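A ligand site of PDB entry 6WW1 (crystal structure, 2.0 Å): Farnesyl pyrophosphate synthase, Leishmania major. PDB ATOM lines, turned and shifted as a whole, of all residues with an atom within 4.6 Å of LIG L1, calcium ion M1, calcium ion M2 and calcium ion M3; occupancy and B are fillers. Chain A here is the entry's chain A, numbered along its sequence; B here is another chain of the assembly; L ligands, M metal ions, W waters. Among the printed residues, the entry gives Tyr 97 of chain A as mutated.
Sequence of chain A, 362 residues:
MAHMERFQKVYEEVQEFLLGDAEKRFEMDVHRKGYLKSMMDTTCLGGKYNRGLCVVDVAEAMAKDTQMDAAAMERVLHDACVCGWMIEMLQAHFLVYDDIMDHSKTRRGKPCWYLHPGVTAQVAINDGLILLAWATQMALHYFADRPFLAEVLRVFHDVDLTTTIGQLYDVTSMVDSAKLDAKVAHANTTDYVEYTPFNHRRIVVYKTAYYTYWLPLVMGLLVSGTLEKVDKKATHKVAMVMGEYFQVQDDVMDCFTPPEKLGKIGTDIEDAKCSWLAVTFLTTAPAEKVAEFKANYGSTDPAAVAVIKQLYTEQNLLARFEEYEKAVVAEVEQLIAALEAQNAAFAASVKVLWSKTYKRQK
NZ of Lys 207 is in salt-bridge range of O5 of LIG L1. NZ of Lys 264 lies within salt-bridge range of O1 of LIG L1 (3.0 Å). An oxygen (O1) of LIG L1 lies within salt-bridge range of the guanidinium group (NH1) of Arg 107 (2.8 Å).
The side-chain carboxylate (OD1) of Asp 250 lies within salt-bridge range of the side-chain amino group (NZ) of Lys 264 (2.7 Å). The side-chain carboxylate (OD2) of Asp 98 lies close to the guanidinium group (NH2) of Arg 107, at 3.96 Å. The side-chain carboxylate of Asp 98 lies close to the side-chain amide nitrogen of Gln 167. The guanidinium group of Arg 107 lies within salt-bridge range of the side-chain carboxylate of Asp 99 (2.8 Å). The side-chain carboxylate (OD2) of Asp 170 is in salt-bridge range of the side-chain amino group (NZ) of Lys 207. The side-chain amide oxygen (OE1) of Gln 247 is in hydrogen-bond range of the side-chain hydroxyl (OG1) of Thr 208 (2.7 Å). The side-chain carboxylate (OD2) of Asp 250 sits close to the side-chain amide nitrogen (NE2) of Gln 247.
Residues that only touch LIG L1: Phe 94 (3.6 Å), Thr 163 (3.7 Å), Gln 167 (3.5 Å), Thr 208 (3.3 Å) and Tyr 211 (3.9 Å). Hydrophobic or aromatic side chains within 4 Å of LIG L1: Phe 94. 11 residues have an atom within 4 Å of LIG L1: Phe 94, Asp 98, Asp 102, Arg 107, Thr 163, Gln 167, Lys 207, Thr 208, Tyr 211, Asp 250 and Lys 264. Along chain A the residues within 4 Å of LIG L1 span positions 94 to 264.
Within 4 Å of calcium ion M1: Asp 250.
Within 4 Å of calcium ion M2: Asp 98 and Asp 102. Along chain A the residues within 4 Å of calcium ion M2 span positions 98 to 102.
The nearest printed residue that does not touch calcium ion M3 is Asp 170 (4.03 Å).
Calcium ion M1 is bound by an oxygen (O3) of LIG L1, an oxygen (O6) of LIG L1, water W1, water W3, water W4 and the side-chain carboxylate (OD2) of Asp 250.
Calcium ion M2 is bound by OD2 of Asp 102, O2 of LIG L1, water W7, OD2 of Asp 98, water W2 and O4 of LIG L1.
Calcium ion M3 is bound by O4 of LIG L1 (2.3 Å), water W6 (2.3 Å), water W9 (2.3 Å), OD2 of Asp 102 (2.4 Å), OD1 of Asp 98 (2.4 Å) and water W10 (2.5 Å). Calcium ion M3 has six donor atoms within binding distance. Slightly farther from calcium ion M3 lies OD1 of Asp 102 (2.9 Å).
Water W3 lies within hydrogen-bond range of the side-chain carboxylate of Asp 268 (2.6 Å) and the backbone carbonyl oxygen of Asp 250 (3.3 Å). Water W6 lies within hydrogen-bond range of OE1 of Gln 167 (2.8 Å) and O5 of LIG L1 (2.9 Å). Water W10 lies within hydrogen-bond range of OD1 of Asp 170 (2.6 Å), OD1 of Asp 102 (3.0 Å) and NE2 of Gln 167 (3.4 Å).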
ATOM      1  N   PHE A  94      12.442   1.098  -2.318  1.00  0.00           N
ATOM      2  CA  PHE A  94      12.966   1.985  -3.343  1.00  0.00           C
ATOM      3  C   PHE A  94      14.502   1.945  -3.409  1.00  0.00           C
ATOM      4  O   PHE A  94      15.048   1.880  -4.472  1.00  0.00           O
ATOM      5  CB  PHE A  94      12.515   3.421  -3.072  1.00  0.00           C
ATOM      6  CG  PHE A  94      11.051   3.700  -3.396  1.00  0.00           C
ATOM      7  CD1 PHE A  94      10.360   2.926  -4.301  1.00  0.00           C
ATOM      8  CD2 PHE A  94      10.396   4.745  -2.747  1.00  0.00           C
ATOM      9  CE1 PHE A  94       9.038   3.211  -4.587  1.00  0.00           C
ATOM     10  CE2 PHE A  94       9.041   5.069  -3.027  1.00  0.00           C
ATOM     11  CZ  PHE A  94       8.366   4.281  -3.940  1.00  0.00           C
ATOM     12  N   LEU A  95      15.170   1.944  -2.265  1.00  0.00           N
ATOM     13  CA  LEU A  95      16.632   1.973  -2.259  1.00  0.00           C
ATOM     14  C   LEU A  95      17.256   0.628  -2.618  1.00  0.00           C
ATOM     15  O   LEU A  95      18.373   0.604  -3.191  1.00  0.00           O
ATOM     16  CB  LEU A  95      17.193   2.503  -0.939  1.00  0.00           C
ATOM     17  CG  LEU A  95      16.621   3.815  -0.398  1.00  0.00           C
ATOM     18  CD1 LEU A  95      17.310   4.242   0.910  1.00  0.00           C
ATOM     19  CD2 LEU A  95      16.680   4.897  -1.487  1.00  0.00           C
ATOM     20  N   TYR A  97      16.102  -1.419  -4.849  1.00  0.00           N
ATOM     21  CA  TYR A  97      16.053  -1.281  -6.313  1.00  0.00           C
ATOM     22  C   TYR A  97      16.934  -0.220  -6.895  1.00  0.00           C
ATOM     23  O   TYR A  97      17.504  -0.403  -7.968  1.00  0.00           O
ATOM     24  CB  TYR A  97      14.614  -1.030  -6.814  1.00  0.00           C
ATOM     25  CG  TYR A  97      13.880  -2.314  -6.778  1.00  0.00           C
ATOM     26  CD1 TYR A  97      14.148  -3.298  -7.691  1.00  0.00           C
ATOM     27  CD2 TYR A  97      12.973  -2.605  -5.748  1.00  0.00           C
ATOM     28  CE1 TYR A  97      13.519  -4.525  -7.628  1.00  0.00           C
ATOM     29  CE2 TYR A  97      12.349  -3.853  -5.689  1.00  0.00           C
ATOM     30  CZ  TYR A  97      12.641  -4.782  -6.651  1.00  0.00           C
ATOM     31  OH  TYR A  97      12.056  -5.979  -6.681  1.00  0.00           O
ATOM     32  N   ASP A  98      16.989   0.922  -6.247  1.00  0.00           N
ATOM     33  CA  ASP A  98      17.733   1.985  -6.835  1.00  0.00           C
ATOM     34  C   ASP A  98      19.250   1.661  -6.790  1.00  0.00           C
ATOM     35  O   ASP A  98      19.978   1.934  -7.734  1.00  0.00           O
ATOM     36  CB  ASP A  98      17.454   3.320  -6.156  1.00  0.00           C
ATOM     37  CG  ASP A  98      18.300   4.471  -6.790  1.00  0.00           C
ATOM     38  OD1 ASP A  98      18.123   4.765  -7.976  1.00  0.00           O
ATOM     39  OD2 ASP A  98      19.181   5.003  -6.079  1.00  0.00           O
ATOM     40  N   ASP A  99      19.706   1.115  -5.674  1.00  0.00           N
ATOM     41  CA  ASP A  99      21.052   0.607  -5.562  1.00  0.00           C
ATOM     42  C   ASP A  99      21.426  -0.373  -6.663  1.00  0.00           C
ATOM     43  O   ASP A  99      22.491  -0.261  -7.276  1.00  0.00           O
ATOM     44  CB  ASP A  99      21.262   0.059  -4.143  1.00  0.00           C
ATOM     45  CG  ASP A  99      21.408   1.191  -3.142  1.00  0.00           C
ATOM     46  OD1 ASP A  99      21.607   2.365  -3.626  1.00  0.00           O
ATOM     47  OD2 ASP A  99      21.400   0.921  -1.929  1.00  0.00           O
ATOM     48  N   ASP A 102      21.490   1.673 -10.054  1.00  0.00           N
ATOM     49  CA  ASP A 102      22.625   2.603 -10.134  1.00  0.00           C
ATOM     50  C   ASP A 102      23.967   1.911 -10.006  1.00  0.00           C
ATOM     51  O   ASP A 102      24.985   2.581 -10.106  1.00  0.00           O
ATOM     52  CB  ASP A 102      22.525   3.661  -8.991  1.00  0.00           C
ATOM     53  CG  ASP A 102      21.487   4.763  -9.287  1.00  0.00           C
ATOM     54  OD1 ASP A 102      20.921   4.811 -10.405  1.00  0.00           O
ATOM     55  OD2 ASP A 102      21.231   5.569  -8.375  1.00  0.00           O
ATOM     56  N   SER A 104      25.417   0.825  -7.262  1.00  0.00           N
ATOM     57  CA  SER A 104      26.133   1.512  -6.180  1.00  0.00           C
ATOM     58  C   SER A 104      26.772   0.509  -5.232  1.00  0.00           C
ATOM     59  O   SER A 104      26.474  -0.695  -5.320  1.00  0.00           O
ATOM     60  CB  SER A 104      25.172   2.405  -5.381  1.00  0.00           C
ATOM     61  OG  SER A 104      24.426   3.249  -6.233  1.00  0.00           O
ATOM     62  N   ARG A 107      25.205   1.759   1.082  1.00  0.00           N
ATOM     63  CA  ARG A 107      23.990   2.475   1.492  1.00  0.00           C
ATOM     64  C   ARG A 107      24.048   2.541   3.016  1.00  0.00           C
ATOM     65  O   ARG A 107      24.298   1.507   3.669  1.00  0.00           O
ATOM     66  CB  ARG A 107      22.705   1.702   1.085  1.00  0.00           C
ATOM     67  CG  ARG A 107      21.459   2.282   1.746  1.00  0.00           C
ATOM     68  CD  ARG A 107      21.111   3.649   1.168  1.00  0.00           C
ATOM     69  NE  ARG A 107      20.866   3.608  -0.284  1.00  0.00           N
ATOM     70  CZ  ARG A 107      20.625   4.701  -1.023  1.00  0.00           C
ATOM     71  NH1 ARG A 107      20.548   5.936  -0.419  1.00  0.00           N
ATOM     72  NH2 ARG A 107      20.389   4.567  -2.335  1.00  0.00           N
ATOM     73  N   THR A 163       6.180   7.802  -7.645  1.00  0.00           N
ATOM     74  CA  THR A 163       7.629   7.588  -7.538  1.00  0.00           C
ATOM     75  C   THR A 163       8.232   6.727  -8.693  1.00  0.00           C
ATOM     76  O   THR A 163       9.350   6.991  -9.172  1.00  0.00           O
ATOM     77  CB  THR A 163       7.995   6.992  -6.147  1.00  0.00           C
ATOM     78  OG1 THR A 163       7.397   7.758  -5.102  1.00  0.00           O
ATOM     79  CG2 THR A 163       9.501   7.001  -5.933  1.00  0.00           C
ATOM     80  N   GLN A 167      11.036   7.811 -11.143  1.00  0.00           N
ATOM     81  CA  GLN A 167      12.225   6.999 -11.485  1.00  0.00           C
ATOM     82  C   GLN A 167      12.392   6.746 -12.982  1.00  0.00           C
ATOM     83  O   GLN A 167      13.528   6.738 -13.474  1.00  0.00           O
ATOM     84  CB  GLN A 167      12.231   5.664 -10.712  1.00  0.00           C
ATOM     85  CG  GLN A 167      13.503   4.812 -10.875  1.00  0.00           C
ATOM     86  CD  GLN A 167      14.662   5.320 -10.035  1.00  0.00           C
ATOM     87  OE1 GLN A 167      14.698   6.506  -9.725  1.00  0.00           O
ATOM     88  NE2 GLN A 167      15.583   4.411  -9.582  1.00  0.00           N
ATOM     89  N   ASP A 170      14.052   9.693 -14.293  1.00  0.00           N
ATOM     90  CA  ASP A 170      15.436   9.671 -13.887  1.00  0.00           C
ATOM     91  C   ASP A 170      16.297   8.761 -14.798  1.00  0.00           C
ATOM     92  O   ASP A 170      17.386   9.206 -15.312  1.00  0.00           O
ATOM     93  CB  ASP A 170      15.595   9.311 -12.384  1.00  0.00           C
ATOM     94  CG  ASP A 170      17.072   9.174 -11.985  1.00  0.00           C
ATOM     95  OD1 ASP A 170      17.688   8.170 -12.395  1.00  0.00           O
ATOM     96  OD2 ASP A 170      17.646  10.068 -11.324  1.00  0.00           O
ATOM     97  N   LYS A 207      10.119  11.676  -8.274  1.00  0.00           N
ATOM     98  CA  LYS A 207      10.836  10.560  -7.688  1.00  0.00           C
ATOM     99  C   LYS A 207      11.049  10.783  -6.205  1.00  0.00           C
ATOM    100  O   LYS A 207      11.455   9.856  -5.488  1.00  0.00           O
ATOM    101  CB  LYS A 207      12.179  10.264  -8.386  1.00  0.00           C
ATOM    102  CG  LYS A 207      13.333  11.213  -8.013  1.00  0.00           C
ATOM    103  CD  LYS A 207      14.706  10.808  -8.614  1.00  0.00           C
ATOM    104  CE  LYS A 207      15.834  11.661  -8.000  1.00  0.00           C
ATOM    105  NZ  LYS A 207      17.191  11.321  -8.619  1.00  0.00           N
ATOM    106  N   THR A 208      10.861  12.013  -5.740  1.00  0.00           N
ATOM    107  CA  THR A 208      11.292  12.348  -4.405  1.00  0.00           C
ATOM    108  C   THR A 208      10.227  13.040  -3.581  1.00  0.00           C
ATOM    109  O   THR A 208       9.941  12.538  -2.534  1.00  0.00           O
ATOM    110  CB  THR A 208      12.619  13.130  -4.354  1.00  0.00           C
ATOM    111  OG1 THR A 208      13.661  12.220  -4.719  1.00  0.00           O
ATOM    112  CG2 THR A 208      12.922  13.568  -2.888  1.00  0.00           C
ATOM    113  N   TYR A 211       6.794  11.064  -2.184  1.00  0.00           N
ATOM    114  CA  TYR A 211       6.928  10.050  -1.128  1.00  0.00           C
ATOM    115  C   TYR A 211       7.699  10.518   0.116  1.00  0.00           C
ATOM    116  O   TYR A 211       7.545   9.903   1.216  1.00  0.00           O
ATOM    117  CB  TYR A 211       7.544   8.747  -1.677  1.00  0.00           C
ATOM    118  CG  TYR A 211       9.073   8.576  -1.589  1.00  0.00           C
ATOM    119  CD1 TYR A 211       9.909   9.038  -2.593  1.00  0.00           C
ATOM    120  CD2 TYR A 211       9.654   7.793  -0.539  1.00  0.00           C
ATOM    121  CE1 TYR A 211      11.297   8.828  -2.546  1.00  0.00           C
ATOM    122  CE2 TYR A 211      11.041   7.573  -0.492  1.00  0.00           C
ATOM    123  CZ  TYR A 211      11.846   8.095  -1.521  1.00  0.00           C
ATOM    124  OH  TYR A 211      13.185   7.865  -1.499  1.00  0.00           O
ATOM    125  N   GLN A 247      15.773  17.244  -2.761  1.00  0.00           N
ATOM    126  CA  GLN A 247      16.458  16.519  -3.861  1.00  0.00           C
ATOM    127  C   GLN A 247      17.664  17.348  -4.322  1.00  0.00           C
ATOM    128  O   GLN A 247      18.713  16.745  -4.638  1.00  0.00           O
ATOM    129  CB  GLN A 247      15.487  16.274  -5.019  1.00  0.00           C
ATOM    130  CG  GLN A 247      15.907  15.119  -5.928  1.00  0.00           C
ATOM    131  CD  GLN A 247      16.612  14.028  -5.159  1.00  0.00           C
ATOM    132  OE1 GLN A 247      16.041  13.377  -4.288  1.00  0.00           O
ATOM    133  NE2 GLN A 247      17.875  13.815  -5.485  1.00  0.00           N
ATOM    134  N   ASP A 250      20.444  16.742  -2.050  1.00  0.00           N
ATOM    135  CA  ASP A 250      20.941  15.367  -2.302  1.00  0.00           C
ATOM    136  C   ASP A 250      21.825  15.385  -3.557  1.00  0.00           C
ATOM    137  O   ASP A 250      22.766  14.572  -3.629  1.00  0.00           O
ATOM    138  CB  ASP A 250      19.786  14.369  -2.427  1.00  0.00           C
ATOM    139  CG  ASP A 250      20.247  12.921  -2.474  1.00  0.00           C
ATOM    140  OD1 ASP A 250      20.959  12.507  -1.532  1.00  0.00           O
ATOM    141  OD2 ASP A 250      19.874  12.214  -3.433  1.00  0.00           O
ATOM    142  N   LYS A 264      27.014   6.974   1.659  1.00  0.00           N
ATOM    143  CA  LYS A 264      26.803   6.422   0.328  1.00  0.00           C
ATOM    144  C   LYS A 264      27.807   7.070  -0.654  1.00  0.00           C
ATOM    145  O   LYS A 264      28.322   8.141  -0.365  1.00  0.00           O
ATOM    146  CB  LYS A 264      25.358   6.664  -0.106  1.00  0.00           C
ATOM    147  CG  LYS A 264      24.969   8.135  -0.186  1.00  0.00           C
ATOM    148  CD  LYS A 264      23.480   8.256  -0.406  1.00  0.00           C
ATOM    149  CE  LYS A 264      23.151   9.711  -0.765  1.00  0.00           C
ATOM    150  NZ  LYS A 264      21.686  10.012  -0.682  1.00  0.00           N
ATOM    151  N   ASP A 268      26.485  10.214  -9.692  1.00  0.00           N
ATOM    152  CA  ASP A 268      25.817  11.162 -10.623  1.00  0.00           C
ATOM    153  C   ASP A 268      26.706  11.539 -11.811  1.00  0.00           C
ATOM    154  O   ASP A 268      26.248  11.582 -12.987  1.00  0.00           O
ATOM    155  CB  ASP A 268      25.297  12.401  -9.881  1.00  0.00           C
ATOM    156  CG  ASP A 268      23.999  12.120  -9.097  1.00  0.00           C
ATOM    157  OD1 ASP A 268      23.569  10.939  -9.017  1.00  0.00           O
ATOM    158  OD2 ASP A 268      23.443  13.100  -8.519  1.00  0.00           O
ATOM    159  N   ASN B 126      12.768  -0.987 -13.155  1.00  0.00           N
ATOM    160  CA  ASN B 126      11.763  -0.013 -12.767  1.00  0.00           C
ATOM    161  C   ASN B 126      10.423  -0.199 -13.508  1.00  0.00           C
ATOM    162  O   ASN B 126       9.345   0.011 -12.923  1.00  0.00           O
ATOM    163  CB  ASN B 126      12.291   1.381 -12.868  1.00  0.00           C
ATOM    164  CG  ASN B 126      11.270   2.421 -12.379  1.00  0.00           C
ATOM    165  OD1 ASN B 126      11.010   2.520 -11.174  1.00  0.00           O
ATOM    166  ND2 ASN B 126      10.707   3.210 -13.293  1.00  0.00           N
ATOM    167  N   LEU B 129       7.947  -2.279 -11.638  1.00  0.00           N
ATOM    168  CA  LEU B 129       7.261  -1.615 -10.532  1.00  0.00           C
ATOM    169  C   LEU B 129       6.083  -0.789 -11.014  1.00  0.00           C
ATOM    170  O   LEU B 129       5.098  -0.642 -10.289  1.00  0.00           O
ATOM    171  CB  LEU B 129       8.196  -0.725  -9.721  1.00  0.00           C
ATOM    172  CG  LEU B 129       9.437  -1.391  -9.164  1.00  0.00           C
ATOM    173  CD1 LEU B 129      10.239  -0.315  -8.420  1.00  0.00           C
ATOM    174  CD2 LEU B 129       9.078  -2.597  -8.297  1.00  0.00           C
HETATM  175  O1  LIG L   1      20.014   8.000  -2.194  1.00  0.00           O
HETATM  176  P1  LIG L   1      20.523   8.107  -3.628  1.00  0.00           P
HETATM  177  O2  LIG L   1      20.869   6.756  -4.174  1.00  0.00           O
HETATM  178  O3  LIG L   1      21.496   9.240  -3.849  1.00  0.00           O
HETATM  179  C1  LIG L   1      19.066   8.638  -4.587  1.00  0.00           C
HETATM  180  P2  LIG L   1      19.296   9.037  -6.342  1.00  0.00           P
HETATM  181  O4  LIG L   1      19.752   7.813  -7.087  1.00  0.00           O
HETATM  182  O5  LIG L   1      17.910   9.481  -6.804  1.00  0.00           O
HETATM  183  O6  LIG L   1      20.174  10.276  -6.336  1.00  0.00           O
HETATM  184  C2  LIG L   1      18.052   7.514  -4.534  1.00  0.00           C
HETATM  185  N1  LIG L   1      16.632   7.772  -4.824  1.00  0.00           N
HETATM  186  C3  LIG L   1      15.958   6.677  -5.276  1.00  0.00           C
HETATM  187  C4  LIG L   1      14.605   6.671  -5.622  1.00  0.00           C
HETATM  188  C5  LIG L   1      13.910   7.878  -5.443  1.00  0.00           C
HETATM  189  C6  LIG L   1      14.571   9.038  -4.957  1.00  0.00           C
HETATM  190  C7  LIG L   1      15.963   8.952  -4.648  1.00  0.00           C
HETATM  191  C8  LIG L   1      14.010   5.351  -6.152  1.00  0.00           C
HETATM  192  C9  LIG L   1      12.733   5.469  -6.966  1.00  0.00           C
HETATM  193  C10 LIG L   1      12.087   4.121  -7.247  1.00  0.00           C
HETATM  194  C11 LIG L   1      13.075   3.018  -7.652  1.00  0.00           C
HETATM  195  P1  LG2 L   2      17.688   7.698   4.688  1.00  0.00           P
HETATM  196  O1  LG2 L   2      18.880   6.711   4.644  1.00  0.00           O
HETATM  197  O2  LG2 L   2      17.694   8.750   5.796  1.00  0.00           O
HETATM  198  O3  LG2 L   2      16.340   6.992   4.577  1.00  0.00           O
HETATM  199  O4  LG2 L   2      17.685   8.349   3.200  1.00  0.00           O
HETATM  200  P2  LG2 L   2      17.242   9.831   2.674  1.00  0.00           P
HETATM  201  O5  LG2 L   2      18.500  10.711   2.546  1.00  0.00           O
HETATM  202  O6  LG2 L   2      16.094  10.378   3.421  1.00  0.00           O
HETATM  203  O7  LG2 L   2      16.673   9.529   1.217  1.00  0.00           O
HETATM  204  C1  LG2 L   2      17.560   9.003   0.234  1.00  0.00           C
HETATM  205  C2  LG2 L   2      16.665   9.078  -0.979  1.00  0.00           C
HETATM  206  C3  LG2 L   2      16.599  10.365  -1.808  1.00  0.00           C
HETATM  207  C4  LG2 L   2      15.211  10.925  -1.842  1.00  0.00           C
HETATM  208  C5  LG2 L   2      17.595  11.506  -1.490  1.00  0.00           C
HETATM  209 CA    CA M   1      21.753  11.117  -4.999  1.00  0.00          CA
HETATM  210 CA    CA M   2      21.228   6.002  -6.219  1.00  0.00          CA
HETATM  211 CA    CA M   3      19.208   6.690  -8.965  1.00  0.00          CA
HETATM  212  O   HOH W   1      23.592  10.462  -6.493  1.00  0.00           O
HETATM  213  O   HOH W   2      23.304   7.220  -6.361  1.00  0.00           O
HETATM  214  O   HOH W   3      21.878  13.085  -6.488  1.00  0.00           O
HETATM  215  O   HOH W   4      23.401  12.148  -3.389  1.00  0.00           O
HETATM  216  O   HOH W   5      24.232   8.325  -3.951  1.00  0.00           O
HETATM  217  O   HOH W   6      17.108   7.587  -8.789  1.00  0.00           O
HETATM  218  O   HOH W   7      22.358   4.170  -5.653  1.00  0.00           O
HETATM  219  O   HOH W   8      20.900  10.881  -9.040  1.00  0.00           O
HETATM  220  O   HOH W   9      19.567   8.717 -10.046  1.00  0.00           O
HETATM  221  O   HOH W  10      18.239   5.946 -11.114  1.00  0.00           O
